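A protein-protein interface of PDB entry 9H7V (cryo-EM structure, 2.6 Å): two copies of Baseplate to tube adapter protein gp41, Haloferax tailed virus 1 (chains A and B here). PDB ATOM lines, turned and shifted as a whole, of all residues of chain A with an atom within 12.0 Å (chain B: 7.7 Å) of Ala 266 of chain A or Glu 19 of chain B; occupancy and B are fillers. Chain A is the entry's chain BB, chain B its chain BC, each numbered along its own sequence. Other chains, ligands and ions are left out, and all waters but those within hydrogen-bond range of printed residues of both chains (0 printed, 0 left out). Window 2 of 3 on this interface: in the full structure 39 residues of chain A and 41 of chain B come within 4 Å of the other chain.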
ATOM      1  N   GLU A 211      39.956 -30.247   9.674  1.00  0.00           N
ATOM      2  CA  GLU A 211      39.213 -29.183   9.014  1.00  0.00           C
ATOM      3  C   GLU A 211      39.011 -29.569   7.549  1.00  0.00           C
ATOM      4  O   GLU A 211      39.972 -29.927   6.869  1.00  0.00           O
ATOM      5  CB  GLU A 211      39.971 -27.851   9.068  1.00  0.00           C
ATOM      6  CG  GLU A 211      40.516 -27.479  10.438  1.00  0.00           C
ATOM      7  CD  GLU A 211      39.515 -27.137  11.530  1.00  0.00           C
ATOM      8  OE1 GLU A 211      38.388 -26.717  11.204  1.00  0.00           O
ATOM      9  OE2 GLU A 211      39.871 -27.293  12.714  1.00  0.00           O
ATOM     10  N   GLN A 262      29.840 -32.596  12.391  1.00  0.00           N
ATOM     11  CA  GLN A 262      30.155 -31.486  11.502  1.00  0.00           C
ATOM     12  C   GLN A 262      29.831 -30.180  12.225  1.00  0.00           C
ATOM     13  O   GLN A 262      28.695 -29.980  12.653  1.00  0.00           O
ATOM     14  CB  GLN A 262      29.321 -31.571  10.219  1.00  0.00           C
ATOM     15  CG  GLN A 262      29.697 -32.713   9.282  1.00  0.00           C
ATOM     16  CD  GLN A 262      28.741 -32.886   8.124  1.00  0.00           C
ATOM     17  OE1 GLN A 262      28.539 -33.991   7.626  1.00  0.00           O
ATOM     18  NE2 GLN A 262      28.149 -31.792   7.672  1.00  0.00           N
ATOM     19  N   VAL A 263      30.833 -29.301  12.355  1.00  0.00           N
ATOM     20  CA  VAL A 263      30.685 -28.059  13.102  1.00  0.00           C
ATOM     21  C   VAL A 263      30.911 -26.863  12.179  1.00  0.00           C
ATOM     22  O   VAL A 263      31.923 -26.786  11.483  1.00  0.00           O
ATOM     23  CB  VAL A 263      31.576 -28.026  14.362  1.00  0.00           C
ATOM     24  CG1 VAL A 263      31.706 -26.634  14.963  1.00  0.00           C
ATOM     25  CG2 VAL A 263      31.075 -28.998  15.419  1.00  0.00           C
ATOM     26  N   HIS A 264      29.936 -25.943  12.200  1.00  0.00           N
ATOM     27  CA  HIS A 264      29.965 -24.689  11.466  1.00  0.00           C
ATOM     28  C   HIS A 264      30.052 -23.536  12.459  1.00  0.00           C
ATOM     29  O   HIS A 264      29.194 -23.399  13.330  1.00  0.00           O
ATOM     30  CB  HIS A 264      28.709 -24.548  10.598  1.00  0.00           C
ATOM     31  CG  HIS A 264      28.536 -25.654   9.616  1.00  0.00           C
ATOM     32  ND1 HIS A 264      28.079 -26.902   9.985  1.00  0.00           N
ATOM     33  CD2 HIS A 264      28.761 -25.707   8.287  1.00  0.00           C
ATOM     34  CE1 HIS A 264      28.032 -27.679   8.924  1.00  0.00           C
ATOM     35  NE2 HIS A 264      28.440 -26.969   7.869  1.00  0.00           N
ATOM     36  N   GLN A 265      31.099 -22.720  12.312  1.00  0.00           N
ATOM     37  CA  GLN A 265      31.308 -21.562  13.164  1.00  0.00           C
ATOM     38  C   GLN A 265      31.043 -20.293  12.362  1.00  0.00           C
ATOM     39  O   GLN A 265      31.334 -20.241  11.167  1.00  0.00           O
ATOM     40  CB  GLN A 265      32.712 -21.583  13.769  1.00  0.00           C
ATOM     41  CG  GLN A 265      32.880 -22.629  14.862  1.00  0.00           C
ATOM     42  CD  GLN A 265      34.315 -22.784  15.300  1.00  0.00           C
ATOM     43  OE1 GLN A 265      35.054 -23.620  14.784  1.00  0.00           O
ATOM     44  NE2 GLN A 265      34.726 -21.969  16.258  1.00  0.00           N
ATOM     45  N   ALA A 266      30.477 -19.287  13.042  1.00  0.00           N
ATOM     46  CA  ALA A 266      30.172 -17.986  12.467  1.00  0.00           C
ATOM     47  C   ALA A 266      31.435 -17.370  11.872  1.00  0.00           C
ATOM     48  O   ALA A 266      32.493 -17.392  12.498  1.00  0.00           O
ATOM     49  CB  ALA A 266      29.578 -17.088  13.525  1.00  0.00           C
ATOM     50  N   GLY A 267      31.312 -16.860  10.642  1.00  0.00           N
ATOM     51  CA  GLY A 267      32.376 -16.107   9.999  1.00  0.00           C
ATOM     52  C   GLY A 267      33.429 -16.974   9.309  1.00  0.00           C
ATOM     53  O   GLY A 267      34.402 -16.434   8.787  1.00  0.00           O
ATOM     54  N   ARG A 268      33.232 -18.300   9.292  1.00  0.00           N
ATOM     55  CA  ARG A 268      34.204 -19.217   8.709  1.00  0.00           C
ATOM     56  C   ARG A 268      33.622 -19.882   7.466  1.00  0.00           C
ATOM     57  O   ARG A 268      32.456 -20.270   7.457  1.00  0.00           O
ATOM     58  CB  ARG A 268      34.644 -20.277   9.724  1.00  0.00           C
ATOM     59  CG  ARG A 268      35.253 -19.703  10.994  1.00  0.00           C
ATOM     60  CD  ARG A 268      36.026 -20.721  11.805  1.00  0.00           C
ATOM     61  NE  ARG A 268      36.508 -20.096  13.029  1.00  0.00           N
ATOM     62  CZ  ARG A 268      37.371 -20.633  13.884  1.00  0.00           C
ATOM     63  NH1 ARG A 268      37.728 -19.959  14.963  1.00  0.00           N
ATOM     64  NH2 ARG A 268      37.877 -21.835  13.665  1.00  0.00           N
ATOM     65  N   GLY A 269      34.462 -20.033   6.436  1.00  0.00           N
ATOM     66  CA  GLY A 269      34.038 -20.584   5.159  1.00  0.00           C
ATOM     67  C   GLY A 269      34.304 -22.084   5.028  1.00  0.00           C
ATOM     68  O   GLY A 269      34.379 -22.591   3.910  1.00  0.00           O
ATOM     69  N   TRP A 270      34.430 -22.787   6.165  1.00  0.00           N
ATOM     70  CA  TRP A 270      34.779 -24.202   6.159  1.00  0.00           C
ATOM     71  C   TRP A 270      34.109 -24.961   7.307  1.00  0.00           C
ATOM     72  O   TRP A 270      33.512 -24.352   8.193  1.00  0.00           O
ATOM     73  CB  TRP A 270      36.305 -24.381   6.139  1.00  0.00           C
ATOM     74  CG  TRP A 270      36.995 -24.123   7.444  1.00  0.00           C
ATOM     75  CD1 TRP A 270      37.168 -25.009   8.467  1.00  0.00           C
ATOM     76  CD2 TRP A 270      37.642 -22.905   7.857  1.00  0.00           C
ATOM     77  NE1 TRP A 270      37.857 -24.424   9.494  1.00  0.00           N
ATOM     78  CE2 TRP A 270      38.165 -23.136   9.150  1.00  0.00           C
ATOM     79  CE3 TRP A 270      37.824 -21.645   7.272  1.00  0.00           C
ATOM     80  CZ2 TRP A 270      38.854 -22.154   9.862  1.00  0.00           C
ATOM     81  CZ3 TRP A 270      38.505 -20.674   7.976  1.00  0.00           C
ATOM     82  CH2 TRP A 270      39.013 -20.928   9.253  1.00  0.00           C
ATOM     83  N   VAL A 271      34.233 -26.297   7.273  1.00  0.00           N
ATOM     84  CA  VAL A 271      33.605 -27.196   8.232  1.00  0.00           C
ATOM     85  C   VAL A 271      34.685 -27.870   9.081  1.00  0.00           C
ATOM     86  O   VAL A 271      35.665 -28.391   8.551  1.00  0.00           O
ATOM     87  CB  VAL A 271      32.685 -28.226   7.540  1.00  0.00           C
ATOM     88  CG1 VAL A 271      32.026 -29.174   8.534  1.00  0.00           C
ATOM     89  CG2 VAL A 271      31.622 -27.555   6.686  1.00  0.00           C
ATOM     90  N   THR A 272      34.475 -27.841  10.403  1.00  0.00           N
ATOM     91  CA  THR A 272      35.317 -28.519  11.376  1.00  0.00           C
ATOM     92  C   THR A 272      34.711 -29.881  11.702  1.00  0.00           C
ATOM     93  O   THR A 272      33.495 -30.009  11.842  1.00  0.00           O
ATOM     94  CB  THR A 272      35.474 -27.679  12.652  1.00  0.00           C
ATOM     95  OG1 THR A 272      35.898 -26.367  12.279  1.00  0.00           O
ATOM     96  CG2 THR A 272      36.460 -28.250  13.648  1.00  0.00           C
ATOM     97  N   PRO B  16      17.482 -16.208  11.505  1.00  0.00           N
ATOM     98  CA  PRO B  16      18.715 -15.612  10.972  1.00  0.00           C
ATOM     99  C   PRO B  16      20.062 -16.344  10.940  1.00  0.00           C
ATOM    100  O   PRO B  16      20.884 -16.029  10.080  1.00  0.00           O
ATOM    101  CB  PRO B  16      18.841 -14.330  11.805  1.00  0.00           C
ATOM    102  CG  PRO B  16      17.404 -13.907  11.983  1.00  0.00           C
ATOM    103  CD  PRO B  16      16.678 -15.212  12.235  1.00  0.00           C
ATOM    104  N   LEU B  17      20.289 -17.291  11.867  1.00  0.00           N
ATOM    105  CA  LEU B  17      21.550 -18.013  12.035  1.00  0.00           C
ATOM    106  C   LEU B  17      22.745 -17.057  12.013  1.00  0.00           C
ATOM    107  O   LEU B  17      23.704 -17.257  11.267  1.00  0.00           O
ATOM    108  CB  LEU B  17      21.687 -19.133  10.993  1.00  0.00           C
ATOM    109  CG  LEU B  17      20.775 -20.351  11.153  1.00  0.00           C
ATOM    110  CD1 LEU B  17      21.264 -21.495  10.284  1.00  0.00           C
ATOM    111  CD2 LEU B  17      20.681 -20.812  12.602  1.00  0.00           C
ATOM    112  N   VAL B  18      22.656 -16.016  12.848  1.00  0.00           N
ATOM    113  CA  VAL B  18      23.732 -15.064  13.068  1.00  0.00           C
ATOM    114  C   VAL B  18      24.249 -15.253  14.492  1.00  0.00           C
ATOM    115  O   VAL B  18      23.472 -15.524  15.407  1.00  0.00           O
ATOM    116  CB  VAL B  18      23.295 -13.606  12.803  1.00  0.00           C
ATOM    117  CG1 VAL B  18      22.726 -13.414  11.406  1.00  0.00           C
ATOM    118  CG2 VAL B  18      22.320 -13.076  13.847  1.00  0.00           C
ATOM    119  N   GLU B  19      25.571 -15.125  14.655  1.00  0.00           N
ATOM    120  CA  GLU B  19      26.212 -15.148  15.960  1.00  0.00           C
ATOM    121  C   GLU B  19      27.507 -14.344  15.930  1.00  0.00           C
ATOM    122  O   GLU B  19      28.018 -14.005  14.864  1.00  0.00           O
ATOM    123  CB  GLU B  19      26.492 -16.576  16.438  1.00  0.00           C
ATOM    124  CG  GLU B  19      25.515 -17.071  17.493  1.00  0.00           C
ATOM    125  CD  GLU B  19      25.340 -16.218  18.742  1.00  0.00           C
ATOM    126  OE1 GLU B  19      26.275 -15.467  19.102  1.00  0.00           O
ATOM    127  OE2 GLU B  19      24.264 -16.316  19.363  1.00  0.00           O
ATOM    128  N   GLU B  20      28.032 -14.075  17.129  1.00  0.00           N
ATOM    129  CA  GLU B  20      29.227 -13.278  17.341  1.00  0.00           C
ATOM    130  C   GLU B  20      30.467 -14.128  17.076  1.00  0.00           C
ATOM    131  O   GLU B  20      30.450 -15.335  17.312  1.00  0.00           O
ATOM    132  CB  GLU B  20      29.216 -12.789  18.790  1.00  0.00           C
ATOM    133  CG  GLU B  20      30.250 -11.722  19.101  1.00  0.00           C
ATOM    134  CD  GLU B  20      30.126 -11.109  20.485  1.00  0.00           C
ATOM    135  OE1 GLU B  20      29.006 -10.694  20.852  1.00  0.00           O
ATOM    136  OE2 GLU B  20      31.148 -11.048  21.196  1.00  0.00           O
ATOM    137  N   GLY B  21      31.527 -13.475  16.579  1.00  0.00           N
ATOM    138  CA  GLY B  21      32.876 -14.022  16.534  1.00  0.00           C
ATOM    139  C   GLY B  21      32.941 -15.407  15.896  1.00  0.00           C
ATOM    140  O   GLY B  21      32.560 -15.570  14.740  1.00  0.00           O
ATOM    141  N   GLY B  22      33.412 -16.390  16.675  1.00  0.00           N
ATOM    142  CA  GLY B  22      33.592 -17.752  16.195  1.00  0.00           C
ATOM    143  C   GLY B  22      32.710 -18.768  16.922  1.00  0.00           C
ATOM    144  O   GLY B  22      33.147 -19.888  17.176  1.00  0.00           O
ATOM    145  N   GLU B  23      31.469 -18.371  17.236  1.00  0.00           N
ATOM    146  CA  GLU B  23      30.513 -19.227  17.926  1.00  0.00           C
ATOM    147  C   GLU B  23      29.955 -20.273  16.960  1.00  0.00           C
ATOM    148  O   GLU B  23      29.869 -20.020  15.760  1.00  0.00           O
ATOM    149  CB  GLU B  23      29.368 -18.400  18.519  1.00  0.00           C
ATOM    150  CG  GLU B  23      29.777 -17.501  19.677  1.00  0.00           C
ATOM    151  CD  GLU B  23      30.263 -18.165  20.958  1.00  0.00           C
ATOM    152  OE1 GLU B  23      29.956 -19.358  21.175  1.00  0.00           O
ATOM    153  OE2 GLU B  23      30.947 -17.481  21.744  1.00  0.00           O
ATOM    154  N   ILE B  24      29.563 -21.435  17.505  1.00  0.00           N
ATOM    155  CA  ILE B  24      29.039 -22.550  16.726  1.00  0.00           C
ATOM    156  C   ILE B  24      27.579 -22.270  16.378  1.00  0.00           C
ATOM    157  O   ILE B  24      26.732 -22.181  17.266  1.00  0.00           O
ATOM    158  CB  ILE B  24      29.232 -23.900  17.457  1.00  0.00           C
ATOM    159  CG1 ILE B  24      30.712 -24.211  17.703  1.00  0.00           C
ATOM    160  CG2 ILE B  24      28.539 -25.032  16.706  1.00  0.00           C
ATOM    161  CD1 ILE B  24      30.970 -25.309  18.716  1.00  0.00           C
ATOM    162  N   LEU B  25      27.306 -22.139  15.073  1.00  0.00           N
ATOM    163  CA  LEU B  25      25.981 -21.828  14.561  1.00  0.00           C
ATOM    164  C   LEU B  25      25.214 -23.110  14.252  1.00  0.00           C
ATOM    165  O   LEU B  25      24.041 -23.222  14.599  1.00  0.00           O
ATOM    166  CB  LEU B  25      26.112 -20.963  13.304  1.00  0.00           C
ATOM    167  CG  LEU B  25      26.278 -19.461  13.532  1.00  0.00           C
ATOM    168  CD1 LEU B  25      26.600 -18.771  12.223  1.00  0.00           C
ATOM    169  CD2 LEU B  25      25.022 -18.854  14.131  1.00  0.00           C
ATOM    170  N   LEU B  26      25.884 -24.055  13.581  1.00  0.00           N
ATOM    171  CA  LEU B  26      25.261 -25.309  13.194  1.00  0.00           C
ATOM    172  C   LEU B  26      26.198 -26.474  13.486  1.00  0.00           C
ATOM    173  O   LEU B  26      27.303 -26.554  12.952  1.00  0.00           O
ATOM    174  CB  LEU B  26      24.850 -25.246  11.717  1.00  0.00           C
ATOM    175  CG  LEU B  26      24.339 -26.546  11.096  1.00  0.00           C
ATOM    176  CD1 LEU B  26      23.030 -26.999  11.729  1.00  0.00           C
ATOM    177  CD2 LEU B  26      24.170 -26.380   9.599  1.00  0.00           C
ATOM    178  N   VAL B  61      22.121 -22.717  16.553  1.00  0.00           N
ATOM    179  CA  VAL B  61      22.207 -21.533  17.391  1.00  0.00           C
ATOM    180  C   VAL B  61      21.987 -20.326  16.485  1.00  0.00           C
ATOM    181  O   VAL B  61      22.511 -20.282  15.376  1.00  0.00           O
ATOM    182  CB  VAL B  61      23.548 -21.456  18.151  1.00  0.00           C
ATOM    183  CG1 VAL B  61      23.671 -20.199  19.000  1.00  0.00           C
ATOM    184  CG2 VAL B  61      23.789 -22.689  19.009  1.00  0.00           C
ATOM    185  N   GLY B  62      21.185 -19.369  16.962  1.00  0.00           N
ATOM    186  CA  GLY B  62      20.915 -18.153  16.217  1.00  0.00           C
ATOM    187  C   GLY B  62      20.225 -17.098  17.072  1.00  0.00           C
ATOM    188  O   GLY B  62      20.136 -17.234  18.291  1.00  0.00           O
ATOM    189  N   LYS B  63      19.743 -16.049  16.398  1.00  0.00           N
ATOM    190  CA  LYS B  63      19.063 -14.940  17.041  1.00  0.00           C
ATOM    191  C   LYS B  63      17.799 -14.592  16.265  1.00  0.00           C
ATOM    192  O   LYS B  63      17.756 -14.757  15.050  1.00  0.00           O
ATOM    193  CB  LYS B  63      20.003 -13.735  17.141  1.00  0.00           C
ATOM    194  CG  LYS B  63      20.876 -13.717  18.387  1.00  0.00           C
ATOM    195  CD  LYS B  63      22.216 -13.053  18.182  1.00  0.00           C
ATOM    196  CE  LYS B  63      22.946 -12.766  19.478  1.00  0.00           C
ATOM    197  NZ  LYS B  63      23.174 -13.991  20.282  1.00  0.00           N
ATOM    198  N   TYR B  65      14.901 -11.296  15.844  1.00  0.00           N
ATOM    199  CA  TYR B  65      14.861  -9.846  15.969  1.00  0.00           C
ATOM    200  C   TYR B  65      13.455  -9.356  16.326  1.00  0.00           C
ATOM    201  O   TYR B  65      13.189  -8.155  16.268  1.00  0.00           O
ATOM    202  CB  TYR B  65      15.348  -9.172  14.681  1.00  0.00           C
ATOM    203  CG  TYR B  65      16.693  -9.598  14.143  1.00  0.00           C
ATOM    204  CD1 TYR B  65      17.811  -9.707  14.961  1.00  0.00           C
ATOM    205  CD2 TYR B  65      16.857  -9.844  12.786  1.00  0.00           C
ATOM    206  CE1 TYR B  65      19.046 -10.083  14.451  1.00  0.00           C
ATOM    207  CE2 TYR B  65      18.084 -10.216  12.260  1.00  0.00           C
ATOM    208  CZ  TYR B  65      19.182 -10.335  13.095  1.00  0.00           C
ATOM    209  OH  TYR B  65      20.390 -10.700  12.577  1.00  0.00           O
ATOM    210  N   ARG B 118      19.576  -5.754  25.640  1.00  0.00           N
ATOM    211  CA  ARG B 118      19.281  -6.634  24.516  1.00  0.00           C
ATOM    212  C   ARG B 118      17.832  -6.521  24.040  1.00  0.00           C
ATOM    213  O   ARG B 118      17.157  -7.538  23.883  1.00  0.00           O
ATOM    214  CB  ARG B 118      19.605  -8.085  24.894  1.00  0.00           C
ATOM    215  CG  ARG B 118      21.085  -8.384  25.086  1.00  0.00           C
ATOM    216  CD  ARG B 118      21.751  -8.803  23.790  1.00  0.00           C
ATOM    217  NE  ARG B 118      23.103  -9.288  24.022  1.00  0.00           N
ATOM    218  CZ  ARG B 118      23.500 -10.552  23.905  1.00  0.00           C
ATOM    219  NH1 ARG B 118      24.762 -10.865  24.147  1.00  0.00           N
ATOM    220  NH2 ARG B 118      22.651 -11.497  23.539  1.00  0.00           N
ATOM    221  N   VAL B 122      16.606 -11.976  20.659  1.00  0.00           N
ATOM    222  CA  VAL B 122      16.258 -13.219  21.331  1.00  0.00           C
ATOM    223  C   VAL B 122      17.283 -14.273  20.921  1.00  0.00           C
ATOM    224  O   VAL B 122      17.545 -14.440  19.733  1.00  0.00           O
ATOM    225  CB  VAL B 122      14.822 -13.671  20.991  1.00  0.00           C
ATOM    226  CG1 VAL B 122      14.393 -14.894  21.792  1.00  0.00           C
ATOM    227  CG2 VAL B 122      13.806 -12.550  21.155  1.00  0.00           C
ATOM    228  N   ASP B 123      17.856 -14.975  21.907  1.00  0.00           N
ATOM    229  CA  ASP B 123      18.804 -16.047  21.644  1.00  0.00           C
ATOM    230  C   ASP B 123      18.052 -17.360  21.441  1.00  0.00           C
ATOM    231  O   ASP B 123      17.244 -17.749  22.282  1.00  0.00           O
ATOM    232  CB  ASP B 123      19.848 -16.176  22.758  1.00  0.00           C
ATOM    233  CG  ASP B 123      20.874 -15.054  22.811  1.00  0.00           C
ATOM    234  OD1 ASP B 123      20.887 -14.209  21.890  1.00  0.00           O
ATOM    235  OD2 ASP B 123      21.661 -15.036  23.779  1.00  0.00           O
ATOM    236  N   VAL B 124      18.351 -18.034  20.322  1.00  0.00           N
ATOM    237  CA  VAL B 124      17.686 -19.263  19.918  1.00  0.00           C
ATOM    238  C   VAL B 124      18.702 -20.403  19.939  1.00  0.00           C
ATOM    239  O   VAL B 124      19.793 -20.275  19.387  1.00  0.00           O
ATOM    240  CB  VAL B 124      17.039 -19.128  18.523  1.00  0.00           C
ATOM    241  CG1 VAL B 124      16.260 -20.373  18.121  1.00  0.00           C
ATOM    242  CG2 VAL B 124      16.153 -17.897  18.417  1.00  0.00           C
ATOM    243  N   SER B 125      18.318 -21.508  20.590  1.00  0.00           N
ATOM    244  CA  SER B 125      18.979 -22.796  20.454  1.00  0.00           C
ATOM    245  C   SER B 125      17.935 -23.860  20.119  1.00  0.00           C
ATOM    246  O   SER B 125      16.968 -24.030  20.858  1.00  0.00           O
ATOM    247  CB  SER B 125      19.759 -23.148  21.695  1.00  0.00           C
ATOM    248  OG  SER B 125      20.861 -22.274  21.870  1.00  0.00           O
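Ala 266 of chain A touches just these residues of chain B: Glu 19, Gly 21, Gly 22, Glu 23 and Leu 25. Glu 19 of chain B touches one residue of chain A. No residue of chain A comes within 4 Å of Val 18 of chain B. No residue of chain A comes within 4 Å of Glu 20 of chain B. Gly 21 of chain B touches one residue of chain A. Of the printed residues of chain A, Glu 23 of chain B touches Gln 265 and Ala 266. Leu 25 of chain B touches two residues of chain A. No residue of chain A comes within 4 Å of Gly 62 of chain B. No residue of chain A comes within 4 Å of Lys 63 of chain B. Of the printed residues of chain B, Gln 262 of chain A touches Leu 26. Of the printed residues of chain B, His 264 of chain A touches Ile 24 (3.5 Å), Leu 25 (2.9 Å) and Leu 26 (2.8 Å). Of the printed residues of chain B, Val 263 of chain A touches Ile 24 (3.8 Å) and Leu 26 (3.7 Å). Of the printed residues of chain B, Gln 265 of chain A touches Gly 22 (2.8 Å), Glu 23 (3.3 Å) and Ile 24 (3.9 Å). Glu 211 of chain A touches none of the printed residues of chain B. Pro 16 of chain B touches none of the printed residues of chain A. The nearest printed residue of chain B that does not touch Gln 265 of chain A is Leu 25 of chain B (4.5 Å).
The backbone carbonyl oxygen (O) of Thr 272 of chain A sits at hydrogen-bond distance from the backbone NH (N) of Val 263 of chain A, at 2.8 Å. NZ of Lys 63 of chain B lies within salt-bridge range of OE2 of Glu 19 of chain B (2.7 Å). O of Leu 25 of chain B is in hydrogen-bond range of N of Val 61 of chain B.
No position is printed for both chains. Of the 14 pairs that touch across the chains among the printed residues, none has its exchanged pair printed and touching as well.
Of the 20 printed residues of chain B, 7 touch a printed residue of chain A.
The backbone NH of Leu 25 of chain B is in hydrogen-bond range of the backbone carbonyl oxygen of His 264 of chain A, 2.9 Å away. The backbone NH (N) of His 264 of chain A lies within hydrogen-bond range of the backbone carbonyl oxygen (O) of Leu 26 of chain B, 2.8 Å away. The side-chain amide nitrogen of Gln 265 of chain A is in hydrogen-bond range of the backbone carbonyl oxygen of Gly 22 of chain B (2.8 Å). The backbone carbonyl oxygen (O) of Glu 23 of chain B sits at hydrogen-bond distance from the backbone NH (N) of Ala 266 of chain A. The backbone carbonyl oxygen (O) of Ala 266 of chain A lies close to the backbone carbonyl oxygen (O) of Gly 21 of chain B (2.9 Å).
O of Gln 262 of chain A touches O of Leu 26 of chain B, at 3.7 Å. Ile 24 of chain B touches Val 263 of chain A (CG1 to CG1, 3.8 Å). Leu 26 of chain B touches Val 263 of chain A. CA of Ile 24 of chain B touches O of His 264 of chain A (3.5 Å). Gln 265 of chain A touches Glu 23 of chain B. Gln 265 of chain A touches Ile 24 of chain B. Ala 266 of chain A touches Glu 19 of chain B. Gly 22 of chain B touches Ala 266 of chain A (CA to O, 3.9 Å). CB of Ala 266 of chain A touches CD1 of Leu 25 of chain B (3.7 Å).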
